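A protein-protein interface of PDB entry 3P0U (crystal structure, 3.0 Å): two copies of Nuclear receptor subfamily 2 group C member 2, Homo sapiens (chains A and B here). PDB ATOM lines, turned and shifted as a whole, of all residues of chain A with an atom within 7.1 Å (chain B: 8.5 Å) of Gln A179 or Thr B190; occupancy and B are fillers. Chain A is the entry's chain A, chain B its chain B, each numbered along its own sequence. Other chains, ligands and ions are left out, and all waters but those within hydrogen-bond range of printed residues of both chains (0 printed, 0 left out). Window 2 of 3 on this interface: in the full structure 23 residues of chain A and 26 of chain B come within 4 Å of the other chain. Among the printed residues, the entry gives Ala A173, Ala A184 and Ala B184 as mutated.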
ATOM      1  N   TYR A 147       9.806  26.419 -18.850  1.00  0.00           N
ATOM      2  CA  TYR A 147       8.654  25.945 -18.054  1.00  0.00           C
ATOM      3  C   TYR A 147       7.458  26.845 -18.240  1.00  0.00           C
ATOM      4  O   TYR A 147       6.333  26.355 -18.376  1.00  0.00           O
ATOM      5  CB  TYR A 147       8.970  25.879 -16.549  1.00  0.00           C
ATOM      6  CG  TYR A 147       9.681  24.608 -16.129  1.00  0.00           C
ATOM      7  CD1 TYR A 147      11.072  24.557 -16.049  1.00  0.00           C
ATOM      8  CD2 TYR A 147       8.964  23.475 -15.820  1.00  0.00           C
ATOM      9  CE1 TYR A 147      11.721  23.411 -15.680  1.00  0.00           C
ATOM     10  CE2 TYR A 147       9.590  22.323 -15.456  1.00  0.00           C
ATOM     11  CZ  TYR A 147      10.973  22.287 -15.391  1.00  0.00           C
ATOM     12  OH  TYR A 147      11.626  21.119 -15.036  1.00  0.00           O
ATOM     13  N   ALA A 173       2.504  19.434 -13.445  1.00  0.00           N
ATOM     14  CA  ALA A 173       3.894  19.065 -13.329  1.00  0.00           C
ATOM     15  C   ALA A 173       4.736  20.213 -13.720  1.00  0.00           C
ATOM     16  O   ALA A 173       5.753  20.482 -13.116  1.00  0.00           O
ATOM     17  CB  ALA A 173       4.186  17.947 -14.244  1.00  0.00           C
ATOM     18  N   ALA A 174       4.332  20.891 -14.771  1.00  0.00           N
ATOM     19  CA  ALA A 174       5.173  21.948 -15.320  1.00  0.00           C
ATOM     20  C   ALA A 174       5.326  23.065 -14.302  1.00  0.00           C
ATOM     21  O   ALA A 174       6.425  23.496 -14.019  1.00  0.00           O
ATOM     22  CB  ALA A 174       4.594  22.479 -16.634  1.00  0.00           C
ATOM     23  N   GLN A 175       4.213  23.516 -13.744  1.00  0.00           N
ATOM     24  CA  GLN A 175       4.253  24.561 -12.742  1.00  0.00           C
ATOM     25  C   GLN A 175       4.914  23.992 -11.486  1.00  0.00           C
ATOM     26  O   GLN A 175       5.593  24.689 -10.726  1.00  0.00           O
ATOM     27  CB  GLN A 175       2.832  25.088 -12.450  1.00  0.00           C
ATOM     28  CG  GLN A 175       1.886  24.045 -11.884  1.00  0.00           C
ATOM     29  CD  GLN A 175       0.619  24.633 -11.353  1.00  0.00           C
ATOM     30  OE1 GLN A 175      -0.360  24.793 -12.094  1.00  0.00           O
ATOM     31  NE2 GLN A 175       0.610  24.937 -10.043  1.00  0.00           N
ATOM     32  N   MET A 176       4.717  22.703 -11.285  1.00  0.00           N
ATOM     33  CA  MET A 176       5.269  22.032 -10.127  1.00  0.00           C
ATOM     34  C   MET A 176       6.781  22.065 -10.184  1.00  0.00           C
ATOM     35  O   MET A 176       7.448  22.676  -9.354  1.00  0.00           O
ATOM     36  CB  MET A 176       4.770  20.604 -10.128  1.00  0.00           C
ATOM     37  CG  MET A 176       5.035  19.831  -8.897  1.00  0.00           C
ATOM     38  SD  MET A 176       3.488  19.040  -8.358  1.00  0.00           S
ATOM     39  CE  MET A 176       3.359  17.655  -9.551  1.00  0.00           C
ATOM     40  N   GLU A 177       7.299  21.451 -11.230  1.00  0.00           N
ATOM     41  CA  GLU A 177       8.715  21.434 -11.515  1.00  0.00           C
ATOM     42  C   GLU A 177       9.327  22.813 -11.651  1.00  0.00           C
ATOM     43  O   GLU A 177      10.527  22.961 -11.533  1.00  0.00           O
ATOM     44  CB  GLU A 177       8.951  20.678 -12.811  1.00  0.00           C
ATOM     45  CG  GLU A 177       8.471  19.227 -12.765  1.00  0.00           C
ATOM     46  CD  GLU A 177       8.852  18.415 -13.993  1.00  0.00           C
ATOM     47  OE1 GLU A 177       9.656  18.893 -14.823  1.00  0.00           O
ATOM     48  OE2 GLU A 177       8.341  17.284 -14.117  1.00  0.00           O
ATOM     49  N   LEU A 178       8.505  23.820 -11.920  1.00  0.00           N
ATOM     50  CA  LEU A 178       8.984  25.186 -12.072  1.00  0.00           C
ATOM     51  C   LEU A 178       9.022  25.893 -10.747  1.00  0.00           C
ATOM     52  O   LEU A 178       9.629  26.945 -10.644  1.00  0.00           O
ATOM     53  CB  LEU A 178       8.069  25.960 -13.013  1.00  0.00           C
ATOM     54  CG  LEU A 178       8.387  27.405 -13.425  1.00  0.00           C
ATOM     55  CD1 LEU A 178       7.744  28.413 -12.480  1.00  0.00           C
ATOM     56  CD2 LEU A 178       9.880  27.637 -13.586  1.00  0.00           C
ATOM     57  N   GLN A 179       8.340  25.356  -9.741  1.00  0.00           N
ATOM     58  CA  GLN A 179       8.394  25.967  -8.400  1.00  0.00           C
ATOM     59  C   GLN A 179       9.637  25.507  -7.730  1.00  0.00           C
ATOM     60  O   GLN A 179      10.211  26.231  -6.926  1.00  0.00           O
ATOM     61  CB  GLN A 179       7.194  25.600  -7.514  1.00  0.00           C
ATOM     62  CG  GLN A 179       7.372  25.994  -6.032  1.00  0.00           C
ATOM     63  CD  GLN A 179       6.069  25.966  -5.257  1.00  0.00           C
ATOM     64  OE1 GLN A 179       5.271  25.061  -5.405  1.00  0.00           O
ATOM     65  NE2 GLN A 179       5.851  26.967  -4.433  1.00  0.00           N
ATOM     66  N   ASP A 180      10.021  24.280  -8.067  1.00  0.00           N
ATOM     67  CA  ASP A 180      11.172  23.649  -7.482  1.00  0.00           C
ATOM     68  C   ASP A 180      12.450  24.295  -7.968  1.00  0.00           C
ATOM     69  O   ASP A 180      13.368  24.543  -7.176  1.00  0.00           O
ATOM     70  CB  ASP A 180      11.186  22.170  -7.836  1.00  0.00           C
ATOM     71  CG  ASP A 180      10.169  21.379  -7.049  1.00  0.00           C
ATOM     72  OD1 ASP A 180       9.961  20.204  -7.408  1.00  0.00           O
ATOM     73  OD2 ASP A 180       9.584  21.916  -6.081  1.00  0.00           O
ATOM     74  N   TYR A 181      12.523  24.558  -9.263  1.00  0.00           N
ATOM     75  CA  TYR A 181      13.715  25.164  -9.810  1.00  0.00           C
ATOM     76  C   TYR A 181      13.946  26.555  -9.198  1.00  0.00           C
ATOM     77  O   TYR A 181      15.075  26.930  -8.921  1.00  0.00           O
ATOM     78  CB  TYR A 181      13.651  25.230 -11.333  1.00  0.00           C
ATOM     79  CG  TYR A 181      14.643  26.201 -11.875  1.00  0.00           C
ATOM     80  CD1 TYR A 181      15.969  25.844 -12.072  1.00  0.00           C
ATOM     81  CD2 TYR A 181      14.275  27.503 -12.126  1.00  0.00           C
ATOM     82  CE1 TYR A 181      16.898  26.766 -12.548  1.00  0.00           C
ATOM     83  CE2 TYR A 181      15.198  28.425 -12.593  1.00  0.00           C
ATOM     84  CZ  TYR A 181      16.500  28.054 -12.802  1.00  0.00           C
ATOM     85  OH  TYR A 181      17.374  29.014 -13.245  1.00  0.00           O
ATOM     86  N   VAL A 182      12.874  27.310  -8.984  1.00  0.00           N
ATOM     87  CA  VAL A 182      12.959  28.672  -8.414  1.00  0.00           C
ATOM     88  C   VAL A 182      13.257  28.578  -6.924  1.00  0.00           C
ATOM     89  O   VAL A 182      14.006  29.379  -6.362  1.00  0.00           O
ATOM     90  CB  VAL A 182      11.626  29.485  -8.651  1.00  0.00           C
ATOM     91  CG1 VAL A 182      11.699  30.874  -8.026  1.00  0.00           C
ATOM     92  CG2 VAL A 182      11.320  29.594 -10.140  1.00  0.00           C
ATOM     93  N   GLN A 183      12.669  27.567  -6.306  1.00  0.00           N
ATOM     94  CA  GLN A 183      12.804  27.336  -4.874  1.00  0.00           C
ATOM     95  C   GLN A 183      14.270  27.221  -4.470  1.00  0.00           C
ATOM     96  O   GLN A 183      14.707  27.851  -3.499  1.00  0.00           O
ATOM     97  CB  GLN A 183      12.079  26.042  -4.481  1.00  0.00           C
ATOM     98  CG  GLN A 183      11.867  25.876  -3.001  1.00  0.00           C
ATOM     99  CD  GLN A 183      10.785  26.773  -2.466  1.00  0.00           C
ATOM    100  OE1 GLN A 183      10.899  27.292  -1.354  1.00  0.00           O
ATOM    101  NE2 GLN A 183       9.727  26.965  -3.244  1.00  0.00           N
ATOM    102  N   ALA A 184      15.014  26.397  -5.211  1.00  0.00           N
ATOM    103  CA  ALA A 184      16.442  26.210  -4.988  1.00  0.00           C
ATOM    104  C   ALA A 184      17.243  27.380  -5.573  1.00  0.00           C
ATOM    105  O   ALA A 184      17.763  28.210  -4.834  1.00  0.00           O
ATOM    106  CB  ALA A 184      16.896  24.884  -5.596  1.00  0.00           C
ATOM    107  N   THR A 190      11.642  34.451  -2.298  1.00  0.00           N
ATOM    108  CA  THR A 190      10.541  33.495  -2.173  1.00  0.00           C
ATOM    109  C   THR A 190       9.363  33.942  -3.024  1.00  0.00           C
ATOM    110  O   THR A 190       8.661  33.126  -3.654  1.00  0.00           O
ATOM    111  CB  THR A 190      10.078  33.358  -0.711  1.00  0.00           C
ATOM    112  OG1 THR A 190      11.223  33.437   0.143  1.00  0.00           O
ATOM    113  CG2 THR A 190       9.323  32.008  -0.484  1.00  0.00           C
ATOM    114  N   LEU A 193       8.748  33.251  -7.624  1.00  0.00           N
ATOM    115  CA  LEU A 193       7.912  32.336  -8.394  1.00  0.00           C
ATOM    116  C   LEU A 193       6.583  33.009  -8.733  1.00  0.00           C
ATOM    117  O   LEU A 193       6.224  33.174  -9.896  1.00  0.00           O
ATOM    118  CB  LEU A 193       7.673  31.053  -7.593  1.00  0.00           C
ATOM    119  CG  LEU A 193       7.039  29.830  -8.270  1.00  0.00           C
ATOM    120  CD1 LEU A 193       5.542  29.872  -8.148  1.00  0.00           C
ATOM    121  CD2 LEU A 193       7.465  29.699  -9.688  1.00  0.00           C
ATOM    122  N   LEU A 197       4.656  33.913 -12.199  1.00  0.00           N
ATOM    123  CA  LEU A 197       3.362  33.436 -12.640  1.00  0.00           C
ATOM    124  C   LEU A 197       2.366  34.589 -12.940  1.00  0.00           C
ATOM    125  O   LEU A 197       1.436  34.445 -13.789  1.00  0.00           O
ATOM    126  CB  LEU A 197       2.775  32.526 -11.586  1.00  0.00           C
ATOM    127  CG  LEU A 197       3.583  31.281 -11.297  1.00  0.00           C
ATOM    128  CD1 LEU A 197       2.882  30.487 -10.259  1.00  0.00           C
ATOM    129  CD2 LEU A 197       3.748  30.457 -12.519  1.00  0.00           C
ATOM    130  N   GLN B 179       0.662  35.057  -0.657  1.00  0.00           N
ATOM    131  CA  GLN B 179       1.587  33.964  -0.425  1.00  0.00           C
ATOM    132  C   GLN B 179       1.699  33.656   1.055  1.00  0.00           C
ATOM    133  O   GLN B 179       1.657  32.496   1.460  1.00  0.00           O
ATOM    134  CB  GLN B 179       2.974  34.279  -0.992  1.00  0.00           C
ATOM    135  CG  GLN B 179       3.984  33.144  -0.814  1.00  0.00           C
ATOM    136  CD  GLN B 179       5.055  33.120  -1.891  1.00  0.00           C
ATOM    137  OE1 GLN B 179       4.811  32.723  -3.032  1.00  0.00           O
ATOM    138  NE2 GLN B 179       6.249  33.528  -1.530  1.00  0.00           N
ATOM    139  N   VAL B 182      -1.090  31.608   2.367  1.00  0.00           N
ATOM    140  CA  VAL B 182      -1.296  30.266   1.837  1.00  0.00           C
ATOM    141  C   VAL B 182      -0.372  29.277   2.538  1.00  0.00           C
ATOM    142  O   VAL B 182      -0.836  28.420   3.289  1.00  0.00           O
ATOM    143  CB  VAL B 182      -1.079  30.233   0.303  1.00  0.00           C
ATOM    144  CG1 VAL B 182      -1.010  28.803  -0.201  1.00  0.00           C
ATOM    145  CG2 VAL B 182      -2.182  31.007  -0.415  1.00  0.00           C
ATOM    146  N   GLN B 183       0.933  29.414   2.307  1.00  0.00           N
ATOM    147  CA  GLN B 183       1.940  28.520   2.914  1.00  0.00           C
ATOM    148  C   GLN B 183       2.000  28.625   4.443  1.00  0.00           C
ATOM    149  O   GLN B 183       2.641  27.793   5.101  1.00  0.00           O
ATOM    150  CB  GLN B 183       3.349  28.696   2.284  1.00  0.00           C
ATOM    151  CG  GLN B 183       3.754  30.110   1.775  1.00  0.00           C
ATOM    152  CD  GLN B 183       4.314  31.028   2.857  1.00  0.00           C
ATOM    153  OE1 GLN B 183       3.664  31.288   3.878  1.00  0.00           O
ATOM    154  NE2 GLN B 183       5.523  31.544   2.621  1.00  0.00           N
ATOM    155  N   ALA B 184       1.325  29.633   5.000  1.00  0.00           N
ATOM    156  CA  ALA B 184       1.177  29.772   6.454  1.00  0.00           C
ATOM    157  C   ALA B 184      -0.164  29.215   6.959  1.00  0.00           C
ATOM    158  O   ALA B 184      -0.355  29.038   8.152  1.00  0.00           O
ATOM    159  CB  ALA B 184       1.331  31.233   6.863  1.00  0.00           C
ATOM    160  N   TYR B 186      -1.312  26.408   5.375  1.00  0.00           N
ATOM    161  CA  TYR B 186      -1.273  25.075   4.778  1.00  0.00           C
ATOM    162  C   TYR B 186       0.069  24.390   4.907  1.00  0.00           C
ATOM    163  O   TYR B 186       1.067  24.992   5.282  1.00  0.00           O
ATOM    164  CB  TYR B 186      -1.652  25.140   3.306  1.00  0.00           C
ATOM    165  CG  TYR B 186      -3.129  25.310   3.086  1.00  0.00           C
ATOM    166  CD1 TYR B 186      -4.007  24.243   3.254  1.00  0.00           C
ATOM    167  CD2 TYR B 186      -3.658  26.540   2.723  1.00  0.00           C
ATOM    168  CE1 TYR B 186      -5.377  24.400   3.051  1.00  0.00           C
ATOM    169  CE2 TYR B 186      -5.017  26.708   2.517  1.00  0.00           C
ATOM    170  CZ  TYR B 186      -5.875  25.640   2.677  1.00  0.00           C
ATOM    171  OH  TYR B 186      -7.229  25.812   2.468  1.00  0.00           O
ATOM    172  N   SER B 187       0.061  23.109   4.584  1.00  0.00           N
ATOM    173  CA  SER B 187       1.239  22.281   4.647  1.00  0.00           C
ATOM    174  C   SER B 187       1.138  21.239   3.554  1.00  0.00           C
ATOM    175  O   SER B 187       2.018  21.146   2.704  1.00  0.00           O
ATOM    176  CB  SER B 187       1.320  21.607   6.018  1.00  0.00           C
ATOM    177  OG  SER B 187       2.464  20.773   6.130  1.00  0.00           O
ATOM    178  N   GLU B 188       0.043  20.478   3.584  1.00  0.00           N
ATOM    179  CA  GLU B 188      -0.242  19.416   2.608  1.00  0.00           C
ATOM    180  C   GLU B 188      -0.182  19.925   1.172  1.00  0.00           C
ATOM    181  O   GLU B 188       0.279  19.219   0.277  1.00  0.00           O
ATOM    182  CB  GLU B 188      -1.629  18.799   2.873  1.00  0.00           C
ATOM    183  CG  GLU B 188      -1.962  17.564   2.020  1.00  0.00           C
ATOM    184  CD  GLU B 188      -3.363  17.022   2.277  1.00  0.00           C
ATOM    185  OE1 GLU B 188      -3.688  16.714   3.444  1.00  0.00           O
ATOM    186  OE2 GLU B 188      -4.136  16.897   1.303  1.00  0.00           O
ATOM    187  N   ASP B 189      -0.666  21.146   0.963  1.00  0.00           N
ATOM    188  CA  ASP B 189      -0.626  21.782  -0.342  1.00  0.00           C
ATOM    189  C   ASP B 189       0.352  22.951  -0.222  1.00  0.00           C
ATOM    190  O   ASP B 189       0.016  24.039   0.263  1.00  0.00           O
ATOM    191  CB  ASP B 189      -2.039  22.220  -0.779  1.00  0.00           C
ATOM    192  CG  ASP B 189      -2.200  22.330  -2.313  1.00  0.00           C
ATOM    193  OD1 ASP B 189      -3.296  22.720  -2.776  1.00  0.00           O
ATOM    194  OD2 ASP B 189      -1.242  22.024  -3.058  1.00  0.00           O
ATOM    195  N   THR B 190       1.592  22.678  -0.610  1.00  0.00           N
ATOM    196  CA  THR B 190       2.630  23.703  -0.682  1.00  0.00           C
ATOM    197  C   THR B 190       2.644  24.348  -2.073  1.00  0.00           C
ATOM    198  O   THR B 190       3.029  25.510  -2.217  1.00  0.00           O
ATOM    199  CB  THR B 190       4.027  23.127  -0.321  1.00  0.00           C
ATOM    200  OG1 THR B 190       5.044  23.992  -0.835  1.00  0.00           O
ATOM    201  CG2 THR B 190       4.231  21.718  -0.884  1.00  0.00           C
ATOM    202  N   TYR B 191       2.182  23.594  -3.076  1.00  0.00           N
ATOM    203  CA  TYR B 191       2.105  24.054  -4.470  1.00  0.00           C
ATOM    204  C   TYR B 191       0.778  24.776  -4.792  1.00  0.00           C
ATOM    205  O   TYR B 191       0.398  24.917  -5.956  1.00  0.00           O
ATOM    206  CB  TYR B 191       2.272  22.853  -5.405  1.00  0.00           C
ATOM    207  CG  TYR B 191       3.611  22.160  -5.354  1.00  0.00           C
ATOM    208  CD1 TYR B 191       3.954  21.339  -4.283  1.00  0.00           C
ATOM    209  CD2 TYR B 191       4.524  22.284  -6.403  1.00  0.00           C
ATOM    210  CE1 TYR B 191       5.177  20.688  -4.249  1.00  0.00           C
ATOM    211  CE2 TYR B 191       5.744  21.640  -6.368  1.00  0.00           C
ATOM    212  CZ  TYR B 191       6.059  20.842  -5.300  1.00  0.00           C
ATOM    213  OH  TYR B 191       7.265  20.208  -5.302  1.00  0.00           O
ATOM    214  N   ARG B 192       0.087  25.232  -3.753  1.00  0.00           N
ATOM    215  CA  ARG B 192      -1.200  25.859  -3.901  1.00  0.00           C
ATOM    216  C   ARG B 192      -1.064  27.188  -4.589  1.00  0.00           C
ATOM    217  O   ARG B 192      -1.625  27.409  -5.654  1.00  0.00           O
ATOM    218  CB  ARG B 192      -1.830  26.074  -2.536  1.00  0.00           C
ATOM    219  CG  ARG B 192      -3.116  26.873  -2.602  1.00  0.00           C
ATOM    220  CD  ARG B 192      -3.854  26.875  -1.279  1.00  0.00           C
ATOM    221  NE  ARG B 192      -5.281  27.188  -1.413  1.00  0.00           N
ATOM    222  CZ  ARG B 192      -6.188  26.372  -1.953  1.00  0.00           C
ATOM    223  NH1 ARG B 192      -5.824  25.201  -2.458  1.00  0.00           N
ATOM    224  NH2 ARG B 192      -7.467  26.730  -2.011  1.00  0.00           N
ATOM    225  N   LEU B 193      -0.305  28.073  -3.961  1.00  0.00           N
ATOM    226  CA  LEU B 193      -0.102  29.421  -4.456  1.00  0.00           C
ATOM    227  C   LEU B 193       0.011  29.364  -5.971  1.00  0.00           C
ATOM    228  O   LEU B 193      -0.683  30.085  -6.701  1.00  0.00           O
ATOM    229  CB  LEU B 193       1.168  30.018  -3.835  1.00  0.00           C
ATOM    230  CG  LEU B 193       1.297  31.517  -3.522  1.00  0.00           C
ATOM    231  CD1 LEU B 193       1.903  32.320  -4.663  1.00  0.00           C
ATOM    232  CD2 LEU B 193      -0.059  32.076  -3.098  1.00  0.00           C
ATOM    233  N   ALA B 194       0.871  28.477  -6.452  1.00  0.00           N
ATOM    234  CA  ALA B 194       1.114  28.383  -7.890  1.00  0.00           C
ATOM    235  C   ALA B 194      -0.185  28.076  -8.611  1.00  0.00           C
ATOM    236  O   ALA B 194      -0.592  28.736  -9.563  1.00  0.00           O
ATOM    237  CB  ALA B 194       2.164  27.288  -8.186  1.00  0.00           C
ATOM    238  N   ARG B 195      -0.830  27.047  -8.115  1.00  0.00           N
ATOM    239  CA  ARG B 195      -2.029  26.553  -8.713  1.00  0.00           C
ATOM    240  C   ARG B 195      -3.081  27.662  -8.855  1.00  0.00           C
ATOM    241  O   ARG B 195      -3.647  27.873  -9.943  1.00  0.00           O
ATOM    242  CB  ARG B 195      -2.562  25.413  -7.855  1.00  0.00           C
ATOM    243  CG  ARG B 195      -3.173  24.265  -8.655  1.00  0.00           C
ATOM    244  CD  ARG B 195      -3.272  23.006  -7.801  1.00  0.00           C
ATOM    245  NE  ARG B 195      -2.011  22.760  -7.087  1.00  0.00           N
ATOM    246  CZ  ARG B 195      -1.766  21.693  -6.334  1.00  0.00           C
ATOM    247  NH1 ARG B 195      -2.669  20.731  -6.187  1.00  0.00           N
ATOM    248  NH2 ARG B 195      -0.595  21.593  -5.741  1.00  0.00           N
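Gln A179 touches Thr B190, and with the chains exchanged Thr A190 touches Gln B179. 6 positions are printed for both chains. Of the 8 pairs that touch across the chains among the printed residues, 2 have their exchanged pair printed and touching as well.
The backbone carbonyl oxygen (O) of Thr A190 is in hydrogen-bond range of the side-chain amide nitrogen (NE2) of Gln B179, 3.2 Å away. NE2 of Gln A175 lies close to N of Arg B195, 3.2 Å away. OD2 of Asp A180 sits at hydrogen-bond distance from OH of Tyr B191 (3.0 Å).
Gln A175 touches Ala B194 (NE2 to CB, 3.4 Å). Met A176 touches Tyr B191 (CG to CE2, 3.2 Å). Gln A179 touches Thr B190. Gln A179 touches Tyr B191 (OE1 to CD2, 3.0 Å). CD1 of Leu A197 touches CA of Ala B194, at 3.6 Å.
The backbone carbonyl oxygen (O) of Tyr B191 sits at hydrogen-bond distance from the guanidinium group (NE) of Arg B195 (3.4 Å). The side-chain carboxylate (OD2) of Asp B189 is in salt-bridge range of the guanidinium group (NH2) of Arg B195. The backbone carbonyl oxygen of Gln B179 lies close to the side-chain amide oxygen of Gln B183 (3.4 Å).
Of the 14 printed residues of chain B, 5 touch a printed residue of chain A. Printed residues of chain B that touch a printed residue of chain A: Gln B179, Thr B190, Tyr B191, Ala B194 and Arg B195. Hydrophobic or aromatic side chains of chain B that line the printed part of chain A: Tyr B191 and Ala B194. Along chain B the printed residues that touch a printed residue of chain A span positions 179 to 195. Of the 16 printed residues of chain A, 6 touch a printed residue of chain B. Among the printed residues, no Asp or Glu carboxylate lies within 4 Å of a Lys or Arg side-chain nitrogen of the other chain.
Of chain B, only Thr B190 (3.9 Å) and Tyr B191 (3.0 Å) come within 4 Å of Gln A179. Printed residues of chain B within 4 Å of Leu A197: Ala B194. Of the printed residues of chain A, Gln B179 touches Thr A190 (3.2 Å). Thr B190 touches one residue of chain A. The nearest residue of chain B that does not touch Gln A179 is Ala B194 (4.7 Å). The nearest printed residue of chain A that does not touch Arg B195 is Met A176 (5.5 Å).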
